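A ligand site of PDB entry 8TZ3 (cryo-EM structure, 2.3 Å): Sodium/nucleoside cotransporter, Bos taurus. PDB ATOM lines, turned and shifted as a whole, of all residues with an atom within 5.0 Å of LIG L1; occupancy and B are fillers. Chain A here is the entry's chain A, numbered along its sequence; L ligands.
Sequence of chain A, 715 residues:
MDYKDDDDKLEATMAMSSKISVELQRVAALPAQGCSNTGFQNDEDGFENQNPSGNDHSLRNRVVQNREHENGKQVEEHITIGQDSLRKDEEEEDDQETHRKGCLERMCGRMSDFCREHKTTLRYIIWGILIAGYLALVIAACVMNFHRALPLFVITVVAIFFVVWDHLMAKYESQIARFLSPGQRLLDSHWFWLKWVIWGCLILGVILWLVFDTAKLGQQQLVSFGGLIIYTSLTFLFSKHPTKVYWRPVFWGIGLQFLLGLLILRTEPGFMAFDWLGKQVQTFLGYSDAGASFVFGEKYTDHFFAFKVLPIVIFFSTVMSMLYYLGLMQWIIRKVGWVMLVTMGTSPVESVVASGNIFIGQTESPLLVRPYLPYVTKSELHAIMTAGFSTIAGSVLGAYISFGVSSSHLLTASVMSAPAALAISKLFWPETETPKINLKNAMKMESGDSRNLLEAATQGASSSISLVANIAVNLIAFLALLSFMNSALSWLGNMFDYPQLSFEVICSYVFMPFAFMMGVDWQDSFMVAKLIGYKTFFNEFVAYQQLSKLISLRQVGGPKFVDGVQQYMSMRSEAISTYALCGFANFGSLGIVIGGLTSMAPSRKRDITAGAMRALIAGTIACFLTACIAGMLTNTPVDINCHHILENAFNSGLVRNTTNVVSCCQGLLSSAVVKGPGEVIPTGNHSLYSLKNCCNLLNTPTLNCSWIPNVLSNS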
ATOM      1  N   TRP A 191     -14.254  18.093 -17.982  1.00  0.00           N
ATOM      2  CA  TRP A 191     -13.761  16.759 -17.635  1.00  0.00           C
ATOM      3  C   TRP A 191     -14.309  15.684 -18.576  1.00  0.00           C
ATOM      4  O   TRP A 191     -13.734  14.593 -18.634  1.00  0.00           O
ATOM      5  CB  TRP A 191     -14.132  16.436 -16.189  1.00  0.00           C
ATOM      6  CG  TRP A 191     -13.950  14.995 -15.844  1.00  0.00           C
ATOM      7  CD1 TRP A 191     -14.915  14.053 -15.747  1.00  0.00           C
ATOM      8  CD2 TRP A 191     -12.713  14.336 -15.552  1.00  0.00           C
ATOM      9  NE1 TRP A 191     -14.365  12.840 -15.407  1.00  0.00           N
ATOM     10  CE2 TRP A 191     -13.015  12.991 -15.290  1.00  0.00           C
ATOM     11  CE3 TRP A 191     -11.378  14.752 -15.493  1.00  0.00           C
ATOM     12  CZ2 TRP A 191     -12.034  12.053 -14.964  1.00  0.00           C
ATOM     13  CZ3 TRP A 191     -10.415  13.828 -15.167  1.00  0.00           C
ATOM     14  CH2 TRP A 191     -10.744  12.497 -14.915  1.00  0.00           C
ATOM     15  N   ILE A 198      -5.903  12.879 -20.080  1.00  0.00           N
ATOM     16  CA  ILE A 198      -5.095  12.597 -18.898  1.00  0.00           C
ATOM     17  C   ILE A 198      -4.808  11.114 -18.796  1.00  0.00           C
ATOM     18  O   ILE A 198      -3.689  10.702 -18.463  1.00  0.00           O
ATOM     19  CB  ILE A 198      -5.806  13.129 -17.645  1.00  0.00           C
ATOM     20  CG1 ILE A 198      -5.855  14.661 -17.685  1.00  0.00           C
ATOM     21  CG2 ILE A 198      -5.110  12.654 -16.385  1.00  0.00           C
ATOM     22  CD1 ILE A 198      -6.666  15.269 -16.585  1.00  0.00           C
ATOM     23  N   TRP A 199      -5.804  10.276 -19.091  1.00  0.00           N
ATOM     24  CA  TRP A 199      -5.582   8.836 -19.091  1.00  0.00           C
ATOM     25  C   TRP A 199      -4.569   8.435 -20.154  1.00  0.00           C
ATOM     26  O   TRP A 199      -3.678   7.611 -19.895  1.00  0.00           O
ATOM     27  CB  TRP A 199      -6.910   8.110 -19.319  1.00  0.00           C
ATOM     28  CG  TRP A 199      -7.889   8.284 -18.193  1.00  0.00           C
ATOM     29  CD1 TRP A 199      -7.638   8.809 -16.965  1.00  0.00           C
ATOM     30  CD2 TRP A 199      -9.277   7.946 -18.218  1.00  0.00           C
ATOM     31  NE1 TRP A 199      -8.781   8.809 -16.214  1.00  0.00           N
ATOM     32  CE2 TRP A 199      -9.805   8.285 -16.955  1.00  0.00           C
ATOM     33  CE3 TRP A 199     -10.123   7.378 -19.166  1.00  0.00           C
ATOM     34  CZ2 TRP A 199     -11.131   8.079 -16.624  1.00  0.00           C
ATOM     35  CZ3 TRP A 199     -11.449   7.173 -18.836  1.00  0.00           C
ATOM     36  CH2 TRP A 199     -11.943   7.525 -17.576  1.00  0.00           C
ATOM     37  N   LEU A 202      -1.018   9.192 -18.959  1.00  0.00           N
ATOM     38  CA  LEU A 202      -0.557   8.255 -17.938  1.00  0.00           C
ATOM     39  C   LEU A 202      -0.134   6.934 -18.556  1.00  0.00           C
ATOM     40  O   LEU A 202       0.948   6.413 -18.261  1.00  0.00           O
ATOM     41  CB  LEU A 202      -1.658   8.034 -16.894  1.00  0.00           C
ATOM     42  CG  LEU A 202      -2.077   9.246 -16.063  1.00  0.00           C
ATOM     43  CD1 LEU A 202      -3.340   8.936 -15.282  1.00  0.00           C
ATOM     44  CD2 LEU A 202      -0.969   9.661 -15.134  1.00  0.00           C
ATOM     45  N   GLY A 205       3.065   7.163 -20.347  1.00  0.00           N
ATOM     46  CA  GLY A 205       4.199   7.239 -19.444  1.00  0.00           C
ATOM     47  C   GLY A 205       4.564   5.890 -18.856  1.00  0.00           C
ATOM     48  O   GLY A 205       5.745   5.594 -18.651  1.00  0.00           O
ATOM     49  N   VAL A 206       3.568   5.059 -18.579  1.00  0.00           N
ATOM     50  CA  VAL A 206       3.837   3.709 -18.087  1.00  0.00           C
ATOM     51  C   VAL A 206       4.586   2.904 -19.132  1.00  0.00           C
ATOM     52  O   VAL A 206       5.531   2.178 -18.816  1.00  0.00           O
ATOM     53  CB  VAL A 206       2.522   3.037 -17.667  1.00  0.00           C
ATOM     54  CG1 VAL A 206       2.724   1.559 -17.419  1.00  0.00           C
ATOM     55  CG2 VAL A 206       1.963   3.699 -16.436  1.00  0.00           C
ATOM     56  N   TRP A 209       8.212   4.123 -19.361  1.00  0.00           N
ATOM     57  CA  TRP A 209       9.027   3.699 -18.234  1.00  0.00           C
ATOM     58  C   TRP A 209       9.415   2.239 -18.352  1.00  0.00           C
ATOM     59  O   TRP A 209      10.538   1.847 -18.022  1.00  0.00           O
ATOM     60  CB  TRP A 209       8.288   3.956 -16.920  1.00  0.00           C
ATOM     61  CG  TRP A 209       9.058   3.550 -15.722  1.00  0.00           C
ATOM     62  CD1 TRP A 209       9.009   2.360 -15.077  1.00  0.00           C
ATOM     63  CD2 TRP A 209      10.026   4.339 -15.026  1.00  0.00           C
ATOM     64  NE1 TRP A 209       9.872   2.348 -14.028  1.00  0.00           N
ATOM     65  CE2 TRP A 209      10.513   3.556 -13.963  1.00  0.00           C
ATOM     66  CE3 TRP A 209      10.525   5.633 -15.184  1.00  0.00           C
ATOM     67  CZ2 TRP A 209      11.476   4.017 -13.081  1.00  0.00           C
ATOM     68  CZ3 TRP A 209      11.475   6.086 -14.310  1.00  0.00           C
ATOM     69  CH2 TRP A 209      11.946   5.283 -13.274  1.00  0.00           C
ATOM     70  N   TYR A 246     -15.709  -0.211  -8.167  1.00  0.00           N
ATOM     71  CA  TYR A 246     -15.301   1.183  -8.341  1.00  0.00           C
ATOM     72  C   TYR A 246     -13.791   1.181  -8.528  1.00  0.00           C
ATOM     73  O   TYR A 246     -13.037   0.836  -7.618  1.00  0.00           O
ATOM     74  CB  TYR A 246     -15.733   2.001  -7.124  1.00  0.00           C
ATOM     75  CG  TYR A 246     -15.496   3.494  -7.217  1.00  0.00           C
ATOM     76  CD1 TYR A 246     -15.604   4.157  -8.420  1.00  0.00           C
ATOM     77  CD2 TYR A 246     -15.192   4.223  -6.084  1.00  0.00           C
ATOM     78  CE1 TYR A 246     -15.406   5.517  -8.497  1.00  0.00           C
ATOM     79  CE2 TYR A 246     -14.994   5.584  -6.151  1.00  0.00           C
ATOM     80  CZ  TYR A 246     -15.096   6.225  -7.352  1.00  0.00           C
ATOM     81  OH  TYR A 246     -14.898   7.585  -7.429  1.00  0.00           O
ATOM     82  N   ARG A 248     -11.536   3.582  -9.228  1.00  0.00           N
ATOM     83  CA  ARG A 248     -10.680   4.698  -8.843  1.00  0.00           C
ATOM     84  C   ARG A 248      -9.725   4.346  -7.712  1.00  0.00           C
ATOM     85  O   ARG A 248      -8.532   4.702  -7.809  1.00  0.00           O
ATOM     86  CB  ARG A 248     -11.570   5.886  -8.466  1.00  0.00           C
ATOM     87  CG  ARG A 248     -10.860   7.122  -8.035  1.00  0.00           C
ATOM     88  CD  ARG A 248     -11.809   8.050  -7.365  1.00  0.00           C
ATOM     89  NE  ARG A 248     -11.146   9.250  -6.887  1.00  0.00           N
ATOM     90  CZ  ARG A 248     -11.710  10.140  -6.083  1.00  0.00           C
ATOM     91  NH1 ARG A 248     -12.958   9.998  -5.674  1.00  0.00           N
ATOM     92  NH2 ARG A 248     -11.012  11.188  -5.692  1.00  0.00           N
ATOM     93  N   PHE A 251      -6.613   2.045  -9.015  1.00  0.00           N
ATOM     94  CA  PHE A 251      -5.555   2.635  -9.814  1.00  0.00           C
ATOM     95  C   PHE A 251      -4.772   3.680  -9.034  1.00  0.00           C
ATOM     96  O   PHE A 251      -3.577   3.883  -9.286  1.00  0.00           O
ATOM     97  CB  PHE A 251      -6.152   3.230 -11.093  1.00  0.00           C
ATOM     98  CG  PHE A 251      -6.537   2.212 -12.120  1.00  0.00           C
ATOM     99  CD1 PHE A 251      -5.621   1.287 -12.577  1.00  0.00           C
ATOM    100  CD2 PHE A 251      -7.812   2.182 -12.637  1.00  0.00           C
ATOM    101  CE1 PHE A 251      -5.973   0.355 -13.515  1.00  0.00           C
ATOM    102  CE2 PHE A 251      -8.164   1.250 -13.575  1.00  0.00           C
ATOM    103  CZ  PHE A 251      -7.244   0.337 -14.013  1.00  0.00           C
ATOM    104  N   TRP A 252      -5.418   4.367  -8.094  1.00  0.00           N
ATOM    105  CA  TRP A 252      -4.707   5.313  -7.249  1.00  0.00           C
ATOM    106  C   TRP A 252      -3.847   4.599  -6.215  1.00  0.00           C
ATOM    107  O   TRP A 252      -2.717   5.024  -5.933  1.00  0.00           O
ATOM    108  CB  TRP A 252      -5.681   6.267  -6.570  1.00  0.00           C
ATOM    109  CG  TRP A 252      -5.901   7.548  -7.289  1.00  0.00           C
ATOM    110  CD1 TRP A 252      -7.019   7.920  -7.949  1.00  0.00           C
ATOM    111  CD2 TRP A 252      -4.978   8.628  -7.428  1.00  0.00           C
ATOM    112  NE1 TRP A 252      -6.864   9.160  -8.494  1.00  0.00           N
ATOM    113  CE2 TRP A 252      -5.612   9.625  -8.183  1.00  0.00           C
ATOM    114  CE3 TRP A 252      -3.681   8.861  -6.984  1.00  0.00           C
ATOM    115  CZ2 TRP A 252      -4.999  10.812  -8.507  1.00  0.00           C
ATOM    116  CZ3 TRP A 252      -3.070  10.039  -7.306  1.00  0.00           C
ATOM    117  CH2 TRP A 252      -3.730  11.011  -8.058  1.00  0.00           C
ATOM    118  N   GLY A 255      -0.848   3.426  -8.025  1.00  0.00           N
ATOM    119  CA  GLY A 255      -0.043   4.565  -8.405  1.00  0.00           C
ATOM    120  C   GLY A 255       0.710   5.190  -7.236  1.00  0.00           C
ATOM    121  O   GLY A 255       1.854   5.611  -7.388  1.00  0.00           O
ATOM    122  N   LEU A 256       0.078   5.261  -6.079  1.00  0.00           N
ATOM    123  CA  LEU A 256       0.737   5.834  -4.909  1.00  0.00           C
ATOM    124  C   LEU A 256       1.926   4.986  -4.474  1.00  0.00           C
ATOM    125  O   LEU A 256       2.980   5.520  -4.118  1.00  0.00           O
ATOM    126  CB  LEU A 256      -0.247   5.981  -3.760  1.00  0.00           C
ATOM    127  CG  LEU A 256      -1.363   7.016  -3.867  1.00  0.00           C
ATOM    128  CD1 LEU A 256      -2.292   6.899  -2.673  1.00  0.00           C
ATOM    129  CD2 LEU A 256      -0.819   8.411  -3.967  1.00  0.00           C
ATOM    130  N   PHE A 258       3.731   3.128  -6.444  1.00  0.00           N
ATOM    131  CA  PHE A 258       4.757   3.329  -7.451  1.00  0.00           C
ATOM    132  C   PHE A 258       5.469   4.658  -7.272  1.00  0.00           C
ATOM    133  O   PHE A 258       6.694   4.751  -7.443  1.00  0.00           O
ATOM    134  CB  PHE A 258       4.120   3.210  -8.832  1.00  0.00           C
ATOM    135  CG  PHE A 258       5.079   3.267  -9.961  1.00  0.00           C
ATOM    136  CD1 PHE A 258       5.944   2.223 -10.212  1.00  0.00           C
ATOM    137  CD2 PHE A 258       5.096   4.347 -10.804  1.00  0.00           C
ATOM    138  CE1 PHE A 258       6.811   2.268 -11.264  1.00  0.00           C
ATOM    139  CE2 PHE A 258       5.964   4.401 -11.867  1.00  0.00           C
ATOM    140  CZ  PHE A 258       6.822   3.362 -12.087  1.00  0.00           C
ATOM    141  N   LEU A 259       4.724   5.719  -6.920  1.00  0.00           N
ATOM    142  CA  LEU A 259       5.356   6.996  -6.640  1.00  0.00           C
ATOM    143  C   LEU A 259       6.253   6.925  -5.415  1.00  0.00           C
ATOM    144  O   LEU A 259       7.373   7.443  -5.414  1.00  0.00           O
ATOM    145  CB  LEU A 259       4.302   8.082  -6.464  1.00  0.00           C
ATOM    146  CG  LEU A 259       3.466   8.426  -7.702  1.00  0.00           C
ATOM    147  CD1 LEU A 259       2.396   9.407  -7.322  1.00  0.00           C
ATOM    148  CD2 LEU A 259       4.322   8.983  -8.798  1.00  0.00           C
ATOM    149  N   LEU A 262       9.440   5.054  -6.436  1.00  0.00           N
ATOM    150  CA  LEU A 262      10.321   5.902  -7.212  1.00  0.00           C
ATOM    151  C   LEU A 262      11.063   6.887  -6.323  1.00  0.00           C
ATOM    152  O   LEU A 262      12.297   7.009  -6.397  1.00  0.00           O
ATOM    153  CB  LEU A 262       9.521   6.660  -8.275  1.00  0.00           C
ATOM    154  CG  LEU A 262       8.993   5.900  -9.482  1.00  0.00           C
ATOM    155  CD1 LEU A 262       8.169   6.835 -10.321  1.00  0.00           C
ATOM    156  CD2 LEU A 262      10.106   5.312 -10.289  1.00  0.00           C
HETATM  157  C1  LIG L   1     -11.962  10.431 -11.510  1.00  0.00           C
HETATM  158  P1  LIG L   1     -14.124   9.682 -10.186  1.00  0.00           P
HETATM  159  C2  LIG L   1     -10.491  10.005 -11.599  1.00  0.00           C
HETATM  160  C3  LIG L   1      -9.594  11.031 -10.945  1.00  0.00           C
HETATM  161  C4  LIG L   1       0.350   7.673 -10.302  1.00  0.00           C
HETATM  162  O1  LIG L   1     -12.499  10.081 -10.252  1.00  0.00           O
HETATM  163  C5  LIG L   1       0.694   7.696 -11.805  1.00  0.00           C
HETATM  164  O2  LIG L   1     -14.319   8.296 -10.752  1.00  0.00           O
HETATM  165  C6  LIG L   1       2.120   7.133 -12.009  1.00  0.00           C
HETATM  166  O3  LIG L   1     -14.625   9.704  -8.770  1.00  0.00           O
HETATM  167  C7  LIG L   1       2.453   7.014 -13.506  1.00  0.00           C
HETATM  168  O4  LIG L   1     -14.983  10.750 -11.098  1.00  0.00           O
HETATM  169  C8  LIG L   1       3.915   6.665 -13.744  1.00  0.00           C
HETATM  170  C9  LIG L   1       4.349   7.031 -15.148  1.00  0.00           C
HETATM  171  C10 LIG L   1       5.789   6.633 -15.410  1.00  0.00           C
HETATM  172  C11 LIG L   1       6.844   7.492 -14.737  1.00  0.00           C
HETATM  173  C12 LIG L   1       6.437   8.940 -14.497  1.00  0.00           C
HETATM  174  C13 LIG L   1      -7.977  11.722 -12.543  1.00  0.00           C
HETATM  175  O5  LIG L   1      -9.227  11.955 -11.942  1.00  0.00           O
HETATM  176  C14 LIG L   1      -6.672  11.843 -11.735  1.00  0.00           C
HETATM  177  O6  LIG L   1      -7.927  11.429 -13.693  1.00  0.00           O
HETATM  178  C15 LIG L   1      -5.478  12.358 -12.564  1.00  0.00           C
HETATM  179  C16 LIG L   1      -4.196  12.416 -11.717  1.00  0.00           C
HETATM  180  C17 LIG L   1      -2.909  12.699 -12.507  1.00  0.00           C
HETATM  181  C18 LIG L   1      -1.669  12.299 -11.689  1.00  0.00           C
HETATM  182  C19 LIG L   1      -0.357  12.884 -12.231  1.00  0.00           C
HETATM  183  C20 LIG L   1     -10.459   7.659 -11.853  1.00  0.00           C
HETATM  184  O7  LIG L   1     -10.327   8.759 -10.951  1.00  0.00           O
HETATM  185  C21 LIG L   1      -9.254   7.267 -12.747  1.00  0.00           C
HETATM  186  O8  LIG L   1     -11.483   7.079 -11.943  1.00  0.00           O
HETATM  187  C22 LIG L   1      -8.055   6.730 -11.943  1.00  0.00           C
HETATM  188  C23 LIG L   1      -6.799   7.571 -12.176  1.00  0.00           C
HETATM  189  C24 LIG L   1      -5.531   6.919 -11.605  1.00  0.00           C
HETATM  190  C25 LIG L   1      -4.357   7.903 -11.567  1.00  0.00           C
HETATM  191  C26 LIG L   1      -3.145   7.381 -10.785  1.00  0.00           C
HETATM  192  C27 LIG L   1      -2.003   8.416 -10.810  1.00  0.00           C
HETATM  193  C28 LIG L   1      -0.875   7.995  -9.853  1.00  0.00           C
HETATM  194  C1  LG2 L   2     -15.474   2.250 -15.064  1.00  0.00           C
HETATM  195  P1  LG2 L   2     -15.767   3.327 -12.634  1.00  0.00           P
HETATM  196  C2  LG2 L   2     -13.967   2.335 -15.301  1.00  0.00           C
HETATM  197  C3  LG2 L   2     -13.515   1.190 -16.201  1.00  0.00           C
HETATM  198  C4  LG2 L   2      -2.811   3.526 -14.903  1.00  0.00           C
HETATM  199  O1  LG2 L   2     -15.876   3.368 -14.294  1.00  0.00           O
HETATM  200  C5  LG2 L   2      -2.466   4.381 -13.675  1.00  0.00           C
HETATM  201  O2  LG2 L   2     -14.545   4.094 -12.172  1.00  0.00           O
HETATM  202  C6  LG2 L   2      -1.773   3.468 -12.630  1.00  0.00           C
HETATM  203  O3  LG2 L   2     -15.658   1.907 -12.155  1.00  0.00           O
HETATM  204  C7  LG2 L   2      -0.252   3.591 -12.701  1.00  0.00           C
HETATM  205  O4  LG2 L   2     -17.111   4.008 -11.984  1.00  0.00           O
HETATM  206  C8  LG2 L   2       0.431   2.486 -11.896  1.00  0.00           C
HETATM  207  C9  LG2 L   2       1.734   2.033 -12.527  1.00  0.00           C
HETATM  208  C10 LG2 L   2       2.311   0.837 -11.818  1.00  0.00           C
HETATM  209  C11 LG2 L   2       3.638   0.345 -12.376  1.00  0.00           C
HETATM  210  C12 LG2 L   2       4.039   0.964 -13.704  1.00  0.00           C
HETATM  211  C13 LG2 L   2     -11.970  -0.609 -16.259  1.00  0.00           C
HETATM  212  O5  LG2 L   2     -12.566   0.417 -15.498  1.00  0.00           O
HETATM  213  C14 LG2 L   2     -10.606  -0.369 -16.927  1.00  0.00           C
HETATM  214  O6  LG2 L   2     -12.513  -1.648 -16.378  1.00  0.00           O
HETATM  215  C15 LG2 L   2      -9.612  -1.512 -16.650  1.00  0.00           C
HETATM  216  C16 LG2 L   2      -8.476  -1.547 -17.699  1.00  0.00           C
HETATM  217  C17 LG2 L   2      -7.712  -0.222 -17.805  1.00  0.00           C
HETATM  218  C18 LG2 L   2      -6.214  -0.454 -18.038  1.00  0.00           C
HETATM  219  C19 LG2 L   2      -5.452   0.847 -18.342  1.00  0.00           C
HETATM  220  C20 LG2 L   2     -12.550   4.224 -15.263  1.00  0.00           C
HETATM  221  O7  LG2 L   2     -13.639   3.573 -15.896  1.00  0.00           O
HETATM  222  C21 LG2 L   2     -11.116   3.650 -15.455  1.00  0.00           C
HETATM  223  O8  LG2 L   2     -12.726   5.169 -14.578  1.00  0.00           O
HETATM  224  C22 LG2 L   2     -10.473   4.070 -16.796  1.00  0.00           C
HETATM  225  C23 LG2 L   2      -9.004   3.679 -16.859  1.00  0.00           C
HETATM  226  C24 LG2 L   2      -8.075   4.877 -16.689  1.00  0.00           C
HETATM  227  C25 LG2 L   2      -6.714   4.460 -16.138  1.00  0.00           C
HETATM  228  C26 LG2 L   2      -5.591   5.348 -16.651  1.00  0.00           C
HETATM  229  C27 LG2 L   2      -4.373   5.330 -15.692  1.00  0.00           C
HETATM  230  C28 LG2 L   2      -3.679   3.956 -15.826  1.00  0.00           C
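OH of Tyr 246 sits at hydrogen-bond distance from O3 of LIG L1 (2.5 Å).
NH1 of Arg 248 is in salt-bridge range of O3 of LIG L1 (3.5 Å).
Trp 191 touches LIG L1.
Ile 198 touches LIG L1.
Trp 199 touches LIG L1 (NE1 to O6, 3.7 Å).
Leu 202 touches LIG L1.
O of Gly 205 touches C10 of LIG L1, at 3.4 Å.
Trp 209 touches LIG L1.
Phe 251 touches LIG L1.
Trp 252 touches LIG L1 (CZ2 to C16, 3.7 Å).
Gly 255 touches LIG L1.
Phe 258 touches LIG L1.
Hydrophobic or aromatic side chains that line LIG L1: Trp 191, Ile 198, Leu 202, Trp 209, Tyr 246, Phe 251, Trp 252 and Phe 258.
12 residues have an atom within 4 Å of LIG L1: Trp 191, Ile 198, Trp 199, Leu 202, Gly 205, Trp 209, Tyr 246, Arg 248, Phe 251, Trp 252, Gly 255 and Phe 258.
Along chain A the residues within 4 Å of LIG L1 span positions 191 to 258.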
